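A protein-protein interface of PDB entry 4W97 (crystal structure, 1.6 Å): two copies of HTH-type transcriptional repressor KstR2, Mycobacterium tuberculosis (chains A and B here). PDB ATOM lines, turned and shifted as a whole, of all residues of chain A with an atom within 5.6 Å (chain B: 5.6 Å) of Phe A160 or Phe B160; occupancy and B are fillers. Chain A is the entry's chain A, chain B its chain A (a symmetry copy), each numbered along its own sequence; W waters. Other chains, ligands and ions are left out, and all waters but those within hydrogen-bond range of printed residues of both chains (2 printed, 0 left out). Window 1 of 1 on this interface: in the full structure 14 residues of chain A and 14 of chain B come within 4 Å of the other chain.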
ATOM      1  N   ASP A 155      -7.769 -26.735 -14.942  1.00  0.00           N
ATOM      2  CA  ASP A 155      -6.660 -25.804 -15.261  1.00  0.00           C
ATOM      3  C   ASP A 155      -5.864 -25.532 -13.997  1.00  0.00           C
ATOM      4  O   ASP A 155      -4.624 -25.469 -14.030  1.00  0.00           O
ATOM      5  CB  ASP A 155      -7.224 -24.502 -15.798  1.00  0.00           C
ATOM      6  CG  ASP A 155      -7.650 -24.605 -17.244  1.00  0.00           C
ATOM      7  OD1 ASP A 155      -7.420 -25.666 -17.864  1.00  0.00           O
ATOM      8  OD2 ASP A 155      -8.166 -23.594 -17.779  1.00  0.00           O
ATOM      9  N   LEU A 156      -6.573 -25.303 -12.885  1.00  0.00           N
ATOM     10  CA  LEU A 156      -5.889 -25.034 -11.599  1.00  0.00           C
ATOM     11  C   LEU A 156      -5.050 -26.203 -11.166  1.00  0.00           C
ATOM     12  O   LEU A 156      -3.927 -26.037 -10.708  1.00  0.00           O
ATOM     13  CB  LEU A 156      -6.855 -24.706 -10.462  1.00  0.00           C
ATOM     14  CG  LEU A 156      -7.280 -23.259 -10.253  1.00  0.00           C
ATOM     15  CD1 LEU A 156      -8.050 -23.112  -8.932  1.00  0.00           C
ATOM     16  CD2 LEU A 156      -6.099 -22.283 -10.312  1.00  0.00           C
ATOM     17  N   VAL A 157      -5.596 -27.413 -11.253  1.00  0.00           N
ATOM     18  CA  VAL A 157      -4.828 -28.567 -10.864  1.00  0.00           C
ATOM     19  C   VAL A 157      -3.636 -28.802 -11.800  1.00  0.00           C
ATOM     20  O   VAL A 157      -2.556 -29.177 -11.342  1.00  0.00           O
ATOM     21  CB  VAL A 157      -5.780 -29.850 -10.789  1.00  0.00           C
ATOM     22  CG1 VAL A 157      -4.953 -31.078 -10.535  1.00  0.00           C
ATOM     23  CG2 VAL A 157      -6.899 -29.628  -9.755  1.00  0.00           C
ATOM     24  N   TYR A 158      -3.832 -28.582 -13.130  1.00  0.00           N
ATOM     25  CA  TYR A 158      -2.687 -28.618 -13.993  1.00  0.00           C
ATOM     26  C   TYR A 158      -1.568 -27.666 -13.516  1.00  0.00           C
ATOM     27  O   TYR A 158      -0.406 -28.097 -13.439  1.00  0.00           O
ATOM     28  CB  TYR A 158      -3.134 -28.270 -15.448  1.00  0.00           C
ATOM     29  CG  TYR A 158      -2.005 -27.676 -16.238  1.00  0.00           C
ATOM     30  CD1 TYR A 158      -0.873 -28.428 -16.574  1.00  0.00           C
ATOM     31  CD2 TYR A 158      -2.086 -26.359 -16.581  1.00  0.00           C
ATOM     32  CE1 TYR A 158       0.241 -27.778 -17.279  1.00  0.00           C
ATOM     33  CE2 TYR A 158      -1.035 -25.738 -17.299  1.00  0.00           C
ATOM     34  CZ  TYR A 158       0.099 -26.487 -17.570  1.00  0.00           C
ATOM     35  OH  TYR A 158       1.134 -25.830 -18.296  1.00  0.00           O
ATOM     36  N   ARG A 159      -1.924 -26.437 -13.191  1.00  0.00           N
ATOM     37  CA  ARG A 159      -0.828 -25.485 -12.834  1.00  0.00           C
ATOM     38  C   ARG A 159      -0.227 -25.889 -11.475  1.00  0.00           C
ATOM     39  O   ARG A 159       0.992 -25.801 -11.276  1.00  0.00           O
ATOM     40  CB  ARG A 159      -1.370 -24.085 -12.735  1.00  0.00           C
ATOM     41  CG  ARG A 159      -1.777 -23.599 -14.107  1.00  0.00           C
ATOM     42  CD  ARG A 159      -2.041 -22.101 -14.071  1.00  0.00           C
ATOM     43  NE  ARG A 159      -3.360 -21.774 -13.551  1.00  0.00           N
ATOM     44  CZ  ARG A 159      -4.439 -21.636 -14.325  1.00  0.00           C
ATOM     45  NH1 ARG A 159      -4.332 -21.823 -15.644  1.00  0.00           N
ATOM     46  NH2 ARG A 159      -5.612 -21.317 -13.792  1.00  0.00           N
ATOM     47  N   PHE A 160      -1.078 -26.401 -10.584  1.00  0.00           N
ATOM     48  CA  PHE A 160      -0.586 -26.867  -9.304  1.00  0.00           C
ATOM     49  C   PHE A 160       0.440 -27.991  -9.547  1.00  0.00           C
ATOM     50  O   PHE A 160       1.504 -28.014  -8.902  1.00  0.00           O
ATOM     51  CB  PHE A 160      -1.784 -27.348  -8.448  1.00  0.00           C
ATOM     52  CG  PHE A 160      -1.412 -27.889  -7.066  1.00  0.00           C
ATOM     53  CD1 PHE A 160      -0.915 -29.189  -6.922  1.00  0.00           C
ATOM     54  CD2 PHE A 160      -1.639 -27.136  -5.949  1.00  0.00           C
ATOM     55  CE1 PHE A 160      -0.584 -29.690  -5.621  1.00  0.00           C
ATOM     56  CE2 PHE A 160      -1.353 -27.613  -4.660  1.00  0.00           C
ATOM     57  CZ  PHE A 160      -0.800 -28.904  -4.507  1.00  0.00           C
ATOM     58  N   ILE A 161       0.078 -28.992 -10.355  1.00  0.00           N
ATOM     59  CA  ILE A 161       0.978 -30.097 -10.606  1.00  0.00           C
ATOM     60  C   ILE A 161       2.286 -29.658 -11.315  1.00  0.00           C
ATOM     61  O   ILE A 161       3.356 -30.052 -10.918  1.00  0.00           O
ATOM     62  CB  ILE A 161       0.276 -31.169 -11.392  1.00  0.00           C
ATOM     63  CG1 ILE A 161      -0.737 -31.845 -10.451  1.00  0.00           C
ATOM     64  CG2 ILE A 161       1.320 -32.183 -11.904  1.00  0.00           C
ATOM     65  CD1 ILE A 161      -1.547 -32.885 -11.229  1.00  0.00           C
ATOM     66  N   ARG A 162       2.112 -28.827 -12.307  1.00  0.00           N
ATOM     67  CA  ARG A 162       3.278 -28.344 -13.064  1.00  0.00           C
ATOM     68  C   ARG A 162       4.205 -27.614 -12.136  1.00  0.00           C
ATOM     69  O   ARG A 162       5.444 -27.871 -12.157  1.00  0.00           O
ATOM     70  CB  ARG A 162       2.828 -27.454 -14.165  1.00  0.00           C
ATOM     71  CG  ARG A 162       4.012 -26.868 -14.963  1.00  0.00           C
ATOM     72  CD  ARG A 162       3.511 -25.645 -15.659  1.00  0.00           C
ATOM     73  NE  ARG A 162       3.129 -24.542 -14.782  1.00  0.00           N
ATOM     74  CZ  ARG A 162       2.445 -23.478 -15.183  1.00  0.00           C
ATOM     75  NH1 ARG A 162       2.050 -23.366 -16.453  1.00  0.00           N
ATOM     76  NH2 ARG A 162       2.136 -22.533 -14.313  1.00  0.00           N
ATOM     77  N   ASP A 163       3.662 -26.731 -11.314  1.00  0.00           N
ATOM     78  CA  ASP A 163       4.545 -25.910 -10.509  1.00  0.00           C
ATOM     79  C   ASP A 163       5.171 -26.731  -9.411  1.00  0.00           C
ATOM     80  O   ASP A 163       6.402 -26.596  -9.211  1.00  0.00           O
ATOM     81  CB  ASP A 163       3.814 -24.705  -9.910  1.00  0.00           C
ATOM     82  CG  ASP A 163       3.489 -23.658 -10.964  1.00  0.00           C
ATOM     83  OD1 ASP A 163       3.933 -23.776 -12.143  1.00  0.00           O
ATOM     84  OD2 ASP A 163       2.783 -22.738 -10.614  1.00  0.00           O
ATOM     85  N   THR A 164       4.382 -27.554  -8.735  1.00  0.00           N
ATOM     86  CA  THR A 164       4.822 -28.337  -7.553  1.00  0.00           C
ATOM     87  C   THR A 164       6.065 -29.102  -7.870  1.00  0.00           C
ATOM     88  O   THR A 164       7.125 -29.034  -7.195  1.00  0.00           O
ATOM     89  CB  THR A 164       3.746 -29.392  -7.057  1.00  0.00           C
ATOM     90  OG1 THR A 164       3.228 -30.208  -8.136  1.00  0.00           O
ATOM     91  CG2 THR A 164       2.624 -28.723  -6.409  1.00  0.00           C
ATOM     92  N   THR A 165       5.915 -29.858  -8.942  1.00  0.00           N
ATOM     93  CA  THR A 165       6.958 -30.787  -9.270  1.00  0.00           C
ATOM     94  C   THR A 165       8.185 -30.112  -9.918  1.00  0.00           C
ATOM     95  O   THR A 165       9.312 -30.274  -9.381  1.00  0.00           O
ATOM     96  CB  THR A 165       6.462 -31.844 -10.213  1.00  0.00           C
ATOM     97  OG1 THR A 165       6.030 -31.326 -11.503  1.00  0.00           O
ATOM     98  CG2 THR A 165       5.311 -32.555  -9.522  1.00  0.00           C
ATOM     99  N   TYR A 187       6.027 -36.248  -2.985  1.00  0.00           N
ATOM    100  CA  TYR A 187       5.183 -35.180  -3.535  1.00  0.00           C
ATOM    101  C   TYR A 187       3.935 -35.810  -4.153  1.00  0.00           C
ATOM    102  O   TYR A 187       2.823 -35.273  -4.005  1.00  0.00           O
ATOM    103  CB  TYR A 187       5.914 -34.384  -4.618  1.00  0.00           C
ATOM    104  CG  TYR A 187       6.751 -33.241  -4.083  1.00  0.00           C
ATOM    105  CD1 TYR A 187       7.407 -33.331  -2.841  1.00  0.00           C
ATOM    106  CD2 TYR A 187       6.960 -32.096  -4.840  1.00  0.00           C
ATOM    107  CE1 TYR A 187       8.128 -32.235  -2.355  1.00  0.00           C
ATOM    108  CE2 TYR A 187       7.687 -31.033  -4.388  1.00  0.00           C
ATOM    109  CZ  TYR A 187       8.309 -31.107  -3.155  1.00  0.00           C
ATOM    110  OH  TYR A 187       9.024 -30.036  -2.653  1.00  0.00           O
ATOM    111  N   ILE A 190       1.184 -36.822  -1.757  1.00  0.00           N
ATOM    112  CA  ILE A 190       0.406 -35.695  -1.280  1.00  0.00           C
ATOM    113  C   ILE A 190      -0.591 -35.276  -2.347  1.00  0.00           C
ATOM    114  O   ILE A 190      -1.791 -35.059  -2.041  1.00  0.00           O
ATOM    115  CB  ILE A 190       1.350 -34.492  -0.905  1.00  0.00           C
ATOM    116  CG1 ILE A 190       2.140 -34.854   0.355  1.00  0.00           C
ATOM    117  CG2 ILE A 190       0.486 -33.240  -0.561  1.00  0.00           C
ATOM    118  CD1 ILE A 190       3.395 -33.848   0.585  1.00  0.00           C
ATOM    119  N   VAL A 191      -0.118 -35.135  -3.585  1.00  0.00           N
ATOM    120  CA  VAL A 191      -1.020 -34.739  -4.669  1.00  0.00           C
ATOM    121  C   VAL A 191      -2.132 -35.766  -4.806  1.00  0.00           C
ATOM    122  O   VAL A 191      -3.303 -35.360  -4.913  1.00  0.00           O
ATOM    123  CB  VAL A 191      -0.255 -34.580  -5.951  1.00  0.00           C
ATOM    124  CG1 VAL A 191      -1.235 -34.383  -7.104  1.00  0.00           C
ATOM    125  CG2 VAL A 191       0.688 -33.362  -5.835  1.00  0.00           C
ATOM    126  N   ASP B 155      10.389 -31.867   6.782  1.00  0.00           N
ATOM    127  CA  ASP B 155      11.178 -30.918   5.960  1.00  0.00           C
ATOM    128  C   ASP B 155      10.642 -30.933   4.540  1.00  0.00           C
ATOM    129  O   ASP B 155      10.530 -29.877   3.894  1.00  0.00           O
ATOM    130  CB  ASP B 155      12.637 -31.333   5.959  1.00  0.00           C
ATOM    131  CG  ASP B 155      13.355 -30.941   7.228  1.00  0.00           C
ATOM    132  OD1 ASP B 155      12.742 -30.259   8.079  1.00  0.00           O
ATOM    133  OD2 ASP B 155      14.560 -31.269   7.349  1.00  0.00           O
ATOM    134  N   LEU B 156      10.369 -32.134   4.019  1.00  0.00           N
ATOM    135  CA  LEU B 156       9.836 -32.255   2.642  1.00  0.00           C
ATOM    136  C   LEU B 156       8.502 -31.576   2.507  1.00  0.00           C
ATOM    137  O   LEU B 156       8.242 -30.886   1.529  1.00  0.00           O
ATOM    138  CB  LEU B 156       9.671 -33.703   2.186  1.00  0.00           C
ATOM    139  CG  LEU B 156      10.849 -34.403   1.523  1.00  0.00           C
ATOM    140  CD1 LEU B 156      10.408 -35.751   0.930  1.00  0.00           C
ATOM    141  CD2 LEU B 156      11.531 -33.533   0.462  1.00  0.00           C
ATOM    142  N   VAL B 157       7.604 -31.796   3.463  1.00  0.00           N
ATOM    143  CA  VAL B 157       6.316 -31.158   3.387  1.00  0.00           C
ATOM    144  C   VAL B 157       6.422 -29.636   3.541  1.00  0.00           C
ATOM    145  O   VAL B 157       5.712 -28.895   2.861  1.00  0.00           O
ATOM    146  CB  VAL B 157       5.332 -31.793   4.477  1.00  0.00           C
ATOM    147  CG1 VAL B 157       4.042 -31.024   4.502  1.00  0.00           C
ATOM    148  CG2 VAL B 157       5.152 -33.301   4.224  1.00  0.00           C
ATOM    149  N   TYR B 158       7.320 -29.161   4.449  1.00  0.00           N
ATOM    150  CA  TYR B 158       7.565 -27.747   4.476  1.00  0.00           C
ATOM    151  C   TYR B 158       7.960 -27.199   3.088  1.00  0.00           C
ATOM    152  O   TYR B 158       7.386 -26.186   2.657  1.00  0.00           O
ATOM    153  CB  TYR B 158       8.671 -27.442   5.533  1.00  0.00           C
ATOM    154  CG  TYR B 158       9.413 -26.182   5.198  1.00  0.00           C
ATOM    155  CD1 TYR B 158       8.784 -24.932   5.231  1.00  0.00           C
ATOM    156  CD2 TYR B 158      10.716 -26.289   4.806  1.00  0.00           C
ATOM    157  CE1 TYR B 158       9.532 -23.737   4.815  1.00  0.00           C
ATOM    158  CE2 TYR B 158      11.454 -25.136   4.447  1.00  0.00           C
ATOM    159  CZ  TYR B 158      10.794 -23.918   4.432  1.00  0.00           C
ATOM    160  OH  TYR B 158      11.570 -22.780   4.069  1.00  0.00           O
ATOM    161  N   ARG B 159       8.885 -27.865   2.420  1.00  0.00           N
ATOM    162  CA  ARG B 159       9.345 -27.274   1.126  1.00  0.00           C
ATOM    163  C   ARG B 159       8.218 -27.392   0.084  1.00  0.00           C
ATOM    164  O   ARG B 159       8.011 -26.477  -0.724  1.00  0.00           O
ATOM    165  CB  ARG B 159      10.558 -28.010   0.624  1.00  0.00           C
ATOM    166  CG  ARG B 159      11.733 -27.734   1.533  1.00  0.00           C
ATOM    167  CD  ARG B 159      13.020 -28.219   0.882  1.00  0.00           C
ATOM    168  NE  ARG B 159      13.223 -29.652   1.034  1.00  0.00           N
ATOM    169  CZ  ARG B 159      13.895 -30.192   2.053  1.00  0.00           C
ATOM    170  NH1 ARG B 159      14.399 -29.401   3.004  1.00  0.00           N
ATOM    171  NH2 ARG B 159      14.063 -31.508   2.124  1.00  0.00           N
ATOM    172  N   PHE B 160       7.453 -28.481   0.165  1.00  0.00           N
ATOM    173  CA  PHE B 160       6.329 -28.641  -0.734  1.00  0.00           C
ATOM    174  C   PHE B 160       5.353 -27.468  -0.521  1.00  0.00           C
ATOM    175  O   PHE B 160       4.846 -26.892  -1.501  1.00  0.00           O
ATOM    176  CB  PHE B 160       5.659 -30.012  -0.466  1.00  0.00           C
ATOM    177  CG  PHE B 160       4.437 -30.312  -1.337  1.00  0.00           C
ATOM    178  CD1 PHE B 160       3.191 -29.755  -1.030  1.00  0.00           C
ATOM    179  CD2 PHE B 160       4.534 -31.195  -2.375  1.00  0.00           C
ATOM    180  CE1 PHE B 160       2.051 -30.055  -1.844  1.00  0.00           C
ATOM    181  CE2 PHE B 160       3.426 -31.532  -3.170  1.00  0.00           C
ATOM    182  CZ  PHE B 160       2.175 -30.932  -2.903  1.00  0.00           C
ATOM    183  N   ILE B 161       4.975 -27.200   0.732  1.00  0.00           N
ATOM    184  CA  ILE B 161       4.037 -26.133   1.006  1.00  0.00           C
ATOM    185  C   ILE B 161       4.581 -24.737   0.601  1.00  0.00           C
ATOM    186  O   ILE B 161       3.886 -23.970  -0.023  1.00  0.00           O
ATOM    187  CB  ILE B 161       3.638 -26.152   2.454  1.00  0.00           C
ATOM    188  CG1 ILE B 161       2.731 -27.377   2.668  1.00  0.00           C
ATOM    189  CG2 ILE B 161       2.890 -24.844   2.788  1.00  0.00           C
ATOM    190  CD1 ILE B 161       2.371 -27.497   4.151  1.00  0.00           C
ATOM    191  N   ARG B 162       5.818 -24.514   0.953  1.00  0.00           N
ATOM    192  CA  ARG B 162       6.444 -23.221   0.632  1.00  0.00           C
ATOM    193  C   ARG B 162       6.448 -23.028  -0.857  1.00  0.00           C
ATOM    194  O   ARG B 162       6.061 -21.928  -1.348  1.00  0.00           O
ATOM    195  CB  ARG B 162       7.828 -23.187   1.170  1.00  0.00           C
ATOM    196  CG  ARG B 162       8.559 -21.874   0.816  1.00  0.00           C
ATOM    197  CD  ARG B 162      10.024 -22.142   0.932  1.00  0.00           C
ATOM    198  NE  ARG B 162      10.562 -23.090  -0.040  1.00  0.00           N
ATOM    199  CZ  ARG B 162      11.768 -23.638   0.048  1.00  0.00           C
ATOM    200  NH1 ARG B 162      12.573 -23.343   1.072  1.00  0.00           N
ATOM    201  NH2 ARG B 162      12.166 -24.495  -0.875  1.00  0.00           N
ATOM    202  N   ASP B 163       6.853 -24.049  -1.595  1.00  0.00           N
ATOM    203  CA  ASP B 163       7.004 -23.845  -3.023  1.00  0.00           C
ATOM    204  C   ASP B 163       5.654 -23.741  -3.685  1.00  0.00           C
ATOM    205  O   ASP B 163       5.485 -22.824  -4.525  1.00  0.00           O
ATOM    206  CB  ASP B 163       7.823 -24.963  -3.675  1.00  0.00           C
ATOM    207  CG  ASP B 163       9.296 -24.872  -3.312  1.00  0.00           C
ATOM    208  OD1 ASP B 163       9.737 -23.878  -2.665  1.00  0.00           O
ATOM    209  OD2 ASP B 163       9.998 -25.796  -3.659  1.00  0.00           O
ATOM    210  N   THR B 164       4.727 -24.619  -3.329  1.00  0.00           N
ATOM    211  CA  THR B 164       3.394 -24.721  -3.973  1.00  0.00           C
ATOM    212  C   THR B 164       2.727 -23.385  -4.003  1.00  0.00           C
ATOM    213  O   THR B 164       2.282 -22.844  -5.048  1.00  0.00           O
ATOM    214  CB  THR B 164       2.404 -25.712  -3.226  1.00  0.00           C
ATOM    215  OG1 THR B 164       2.345 -25.469  -1.800  1.00  0.00           O
ATOM    216  CG2 THR B 164       2.802 -27.099  -3.439  1.00  0.00           C
ATOM    217  N   THR B 165       2.660 -22.844  -2.800  1.00  0.00           N
ATOM    218  CA  THR B 165       1.890 -21.644  -2.637  1.00  0.00           C
ATOM    219  C   THR B 165       2.614 -20.387  -3.162  1.00  0.00           C
ATOM    220  O   THR B 165       2.035 -19.681  -4.029  1.00  0.00           O
ATOM    221  CB  THR B 165       1.554 -21.413  -1.193  1.00  0.00           C
ATOM    222  OG1 THR B 165       2.718 -21.206  -0.343  1.00  0.00           O
ATOM    223  CG2 THR B 165       0.766 -22.622  -0.717  1.00  0.00           C
ATOM    224  N   TYR B 187      -5.817 -24.743  -3.723  1.00  0.00           N
ATOM    225  CA  TYR B 187      -4.508 -25.350  -3.453  1.00  0.00           C
ATOM    226  C   TYR B 187      -4.540 -25.988  -2.065  1.00  0.00           C
ATOM    227  O   TYR B 187      -3.999 -27.091  -1.870  1.00  0.00           O
ATOM    228  CB  TYR B 187      -3.386 -24.310  -3.485  1.00  0.00           C
ATOM    229  CG  TYR B 187      -2.818 -24.060  -4.867  1.00  0.00           C
ATOM    230  CD1 TYR B 187      -3.628 -24.123  -6.015  1.00  0.00           C
ATOM    231  CD2 TYR B 187      -1.491 -23.684  -5.032  1.00  0.00           C
ATOM    232  CE1 TYR B 187      -3.056 -23.939  -7.279  1.00  0.00           C
ATOM    233  CE2 TYR B 187      -0.932 -23.472  -6.260  1.00  0.00           C
ATOM    234  CZ  TYR B 187      -1.719 -23.561  -7.393  1.00  0.00           C
ATOM    235  OH  TYR B 187      -1.175 -23.386  -8.652  1.00  0.00           O
ATOM    236  N   ILE B 190      -6.223 -29.369  -1.793  1.00  0.00           N
ATOM    237  CA  ILE B 190      -5.400 -30.452  -2.297  1.00  0.00           C
ATOM    238  C   ILE B 190      -4.352 -30.820  -1.260  1.00  0.00           C
ATOM    239  O   ILE B 190      -4.149 -32.025  -0.966  1.00  0.00           O
ATOM    240  CB  ILE B 190      -4.714 -30.040  -3.653  1.00  0.00           C
ATOM    241  CG1 ILE B 190      -5.783 -29.955  -4.745  1.00  0.00           C
ATOM    242  CG2 ILE B 190      -3.705 -31.149  -4.084  1.00  0.00           C
ATOM    243  CD1 ILE B 190      -5.235 -29.174  -6.060  1.00  0.00           C
ATOM    244  N   VAL B 191      -3.666 -29.814  -0.719  1.00  0.00           N
ATOM    245  CA  VAL B 191      -2.643 -30.089   0.291  1.00  0.00           C
ATOM    246  C   VAL B 191      -3.278 -30.793   1.479  1.00  0.00           C
ATOM    247  O   VAL B 191      -2.708 -31.794   1.948  1.00  0.00           O
ATOM    248  CB  VAL B 191      -1.962 -28.816   0.703  1.00  0.00           C
ATOM    249  CG1 VAL B 191      -1.061 -29.090   1.903  1.00  0.00           C
ATOM    250  CG2 VAL B 191      -1.130 -28.276  -0.481  1.00  0.00           C
HETATM  251  O   HOH W   1       1.266 -22.806  -8.746  1.00  0.00           O
HETATM  252  O   HOH W   2       9.205 -28.018  -4.137  1.00  0.00           O
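OG1 of Thr B164 lies close to O of Phe B160 (2.9 Å).
The side-chain hydroxyl of Thr A164 lies within hydrogen-bond range of the backbone carbonyl oxygen of Ile A161, at 2.8 Å.
The backbone carbonyl oxygen (O) of Phe A160 lies close to the side-chain hydroxyl (OG1) of Thr A164 (2.9 Å).
The backbone carbonyl oxygen (O) of Ile B161 is in hydrogen-bond range of the side-chain hydroxyl (OG1) of Thr B164 (2.8 Å).
Among the printed residues, merely in contact across the chains: Arg A159 with Tyr B187 (3.9 Å), Phe A160 with Phe B160 (3.9 Å), Phe A160 with Tyr B187 (3.5 Å), Phe A160 with Ile B190 (3.7 Å), Thr A164 with Thr B164 (3.4 Å), Tyr A187 with Arg B159 (3.9 Å), Tyr A187 with Phe B160 (3.5 Å), Ile A190 with Phe B160 (3.7 Å) and Ile A190 with Ile B190 (3.99 Å).
Of the printed residues of chain B, Phe A160 touches Phe B160 (3.9 Å), Tyr B187 (3.5 Å) and Ile B190 (3.7 Å).
Of the printed residues of chain A, Phe B160 touches Phe A160, Tyr A187 and Ile A190.
Printed residues of chain B within 4 Å of Thr A164: Thr B164 (3.4 Å).
Of the printed residues of chain A, Tyr B187 touches Arg A159 and Phe A160.
The nearest printed residue of chain B that does not touch Phe A160 is Val B191 (4.1 Å).
Of the 14 printed residues of chain A, 5 touch a printed residue of chain B.
Printed residues of chain B that touch a printed residue of chain A: Arg B159, Phe B160, Thr B164, Tyr B187 and Ile B190.
Among the printed residues, 9 pairs touch across the chains.
Among the printed residues, no Asp or Glu carboxylate lies within 4 Å of a Lys or Arg side-chain nitrogen of the other chain.
Arg A159 touches Tyr B187, and with the chains exchanged Tyr A187 touches Arg B159.
Phe A160 touches its own counterpart, Phe B160.
Phe A160 touches Ile B190, and with the chains exchanged Ile A190 touches Phe B160.
Ile B190 touches its own counterpart, Ile A190.
Positions printed for both chains: 155, 156, 157, 158, 159, 160, 161, 162, 163, 164, 165, 187, 190 and 191.
Of the 9 pairs that touch across the chains among the printed residues, 9 have their exchanged pair printed and touching as well.
Water W1 lies within hydrogen-bond range of OD2 of Asp A163 (2.4 Å) and OH of Tyr B187 (2.5 Å).
Water W2 lies within hydrogen-bond range of the side-chain carboxylate (OD2) of Asp B163 (2.4 Å) and the side-chain hydroxyl (OH) of Tyr A187 (2.5 Å).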
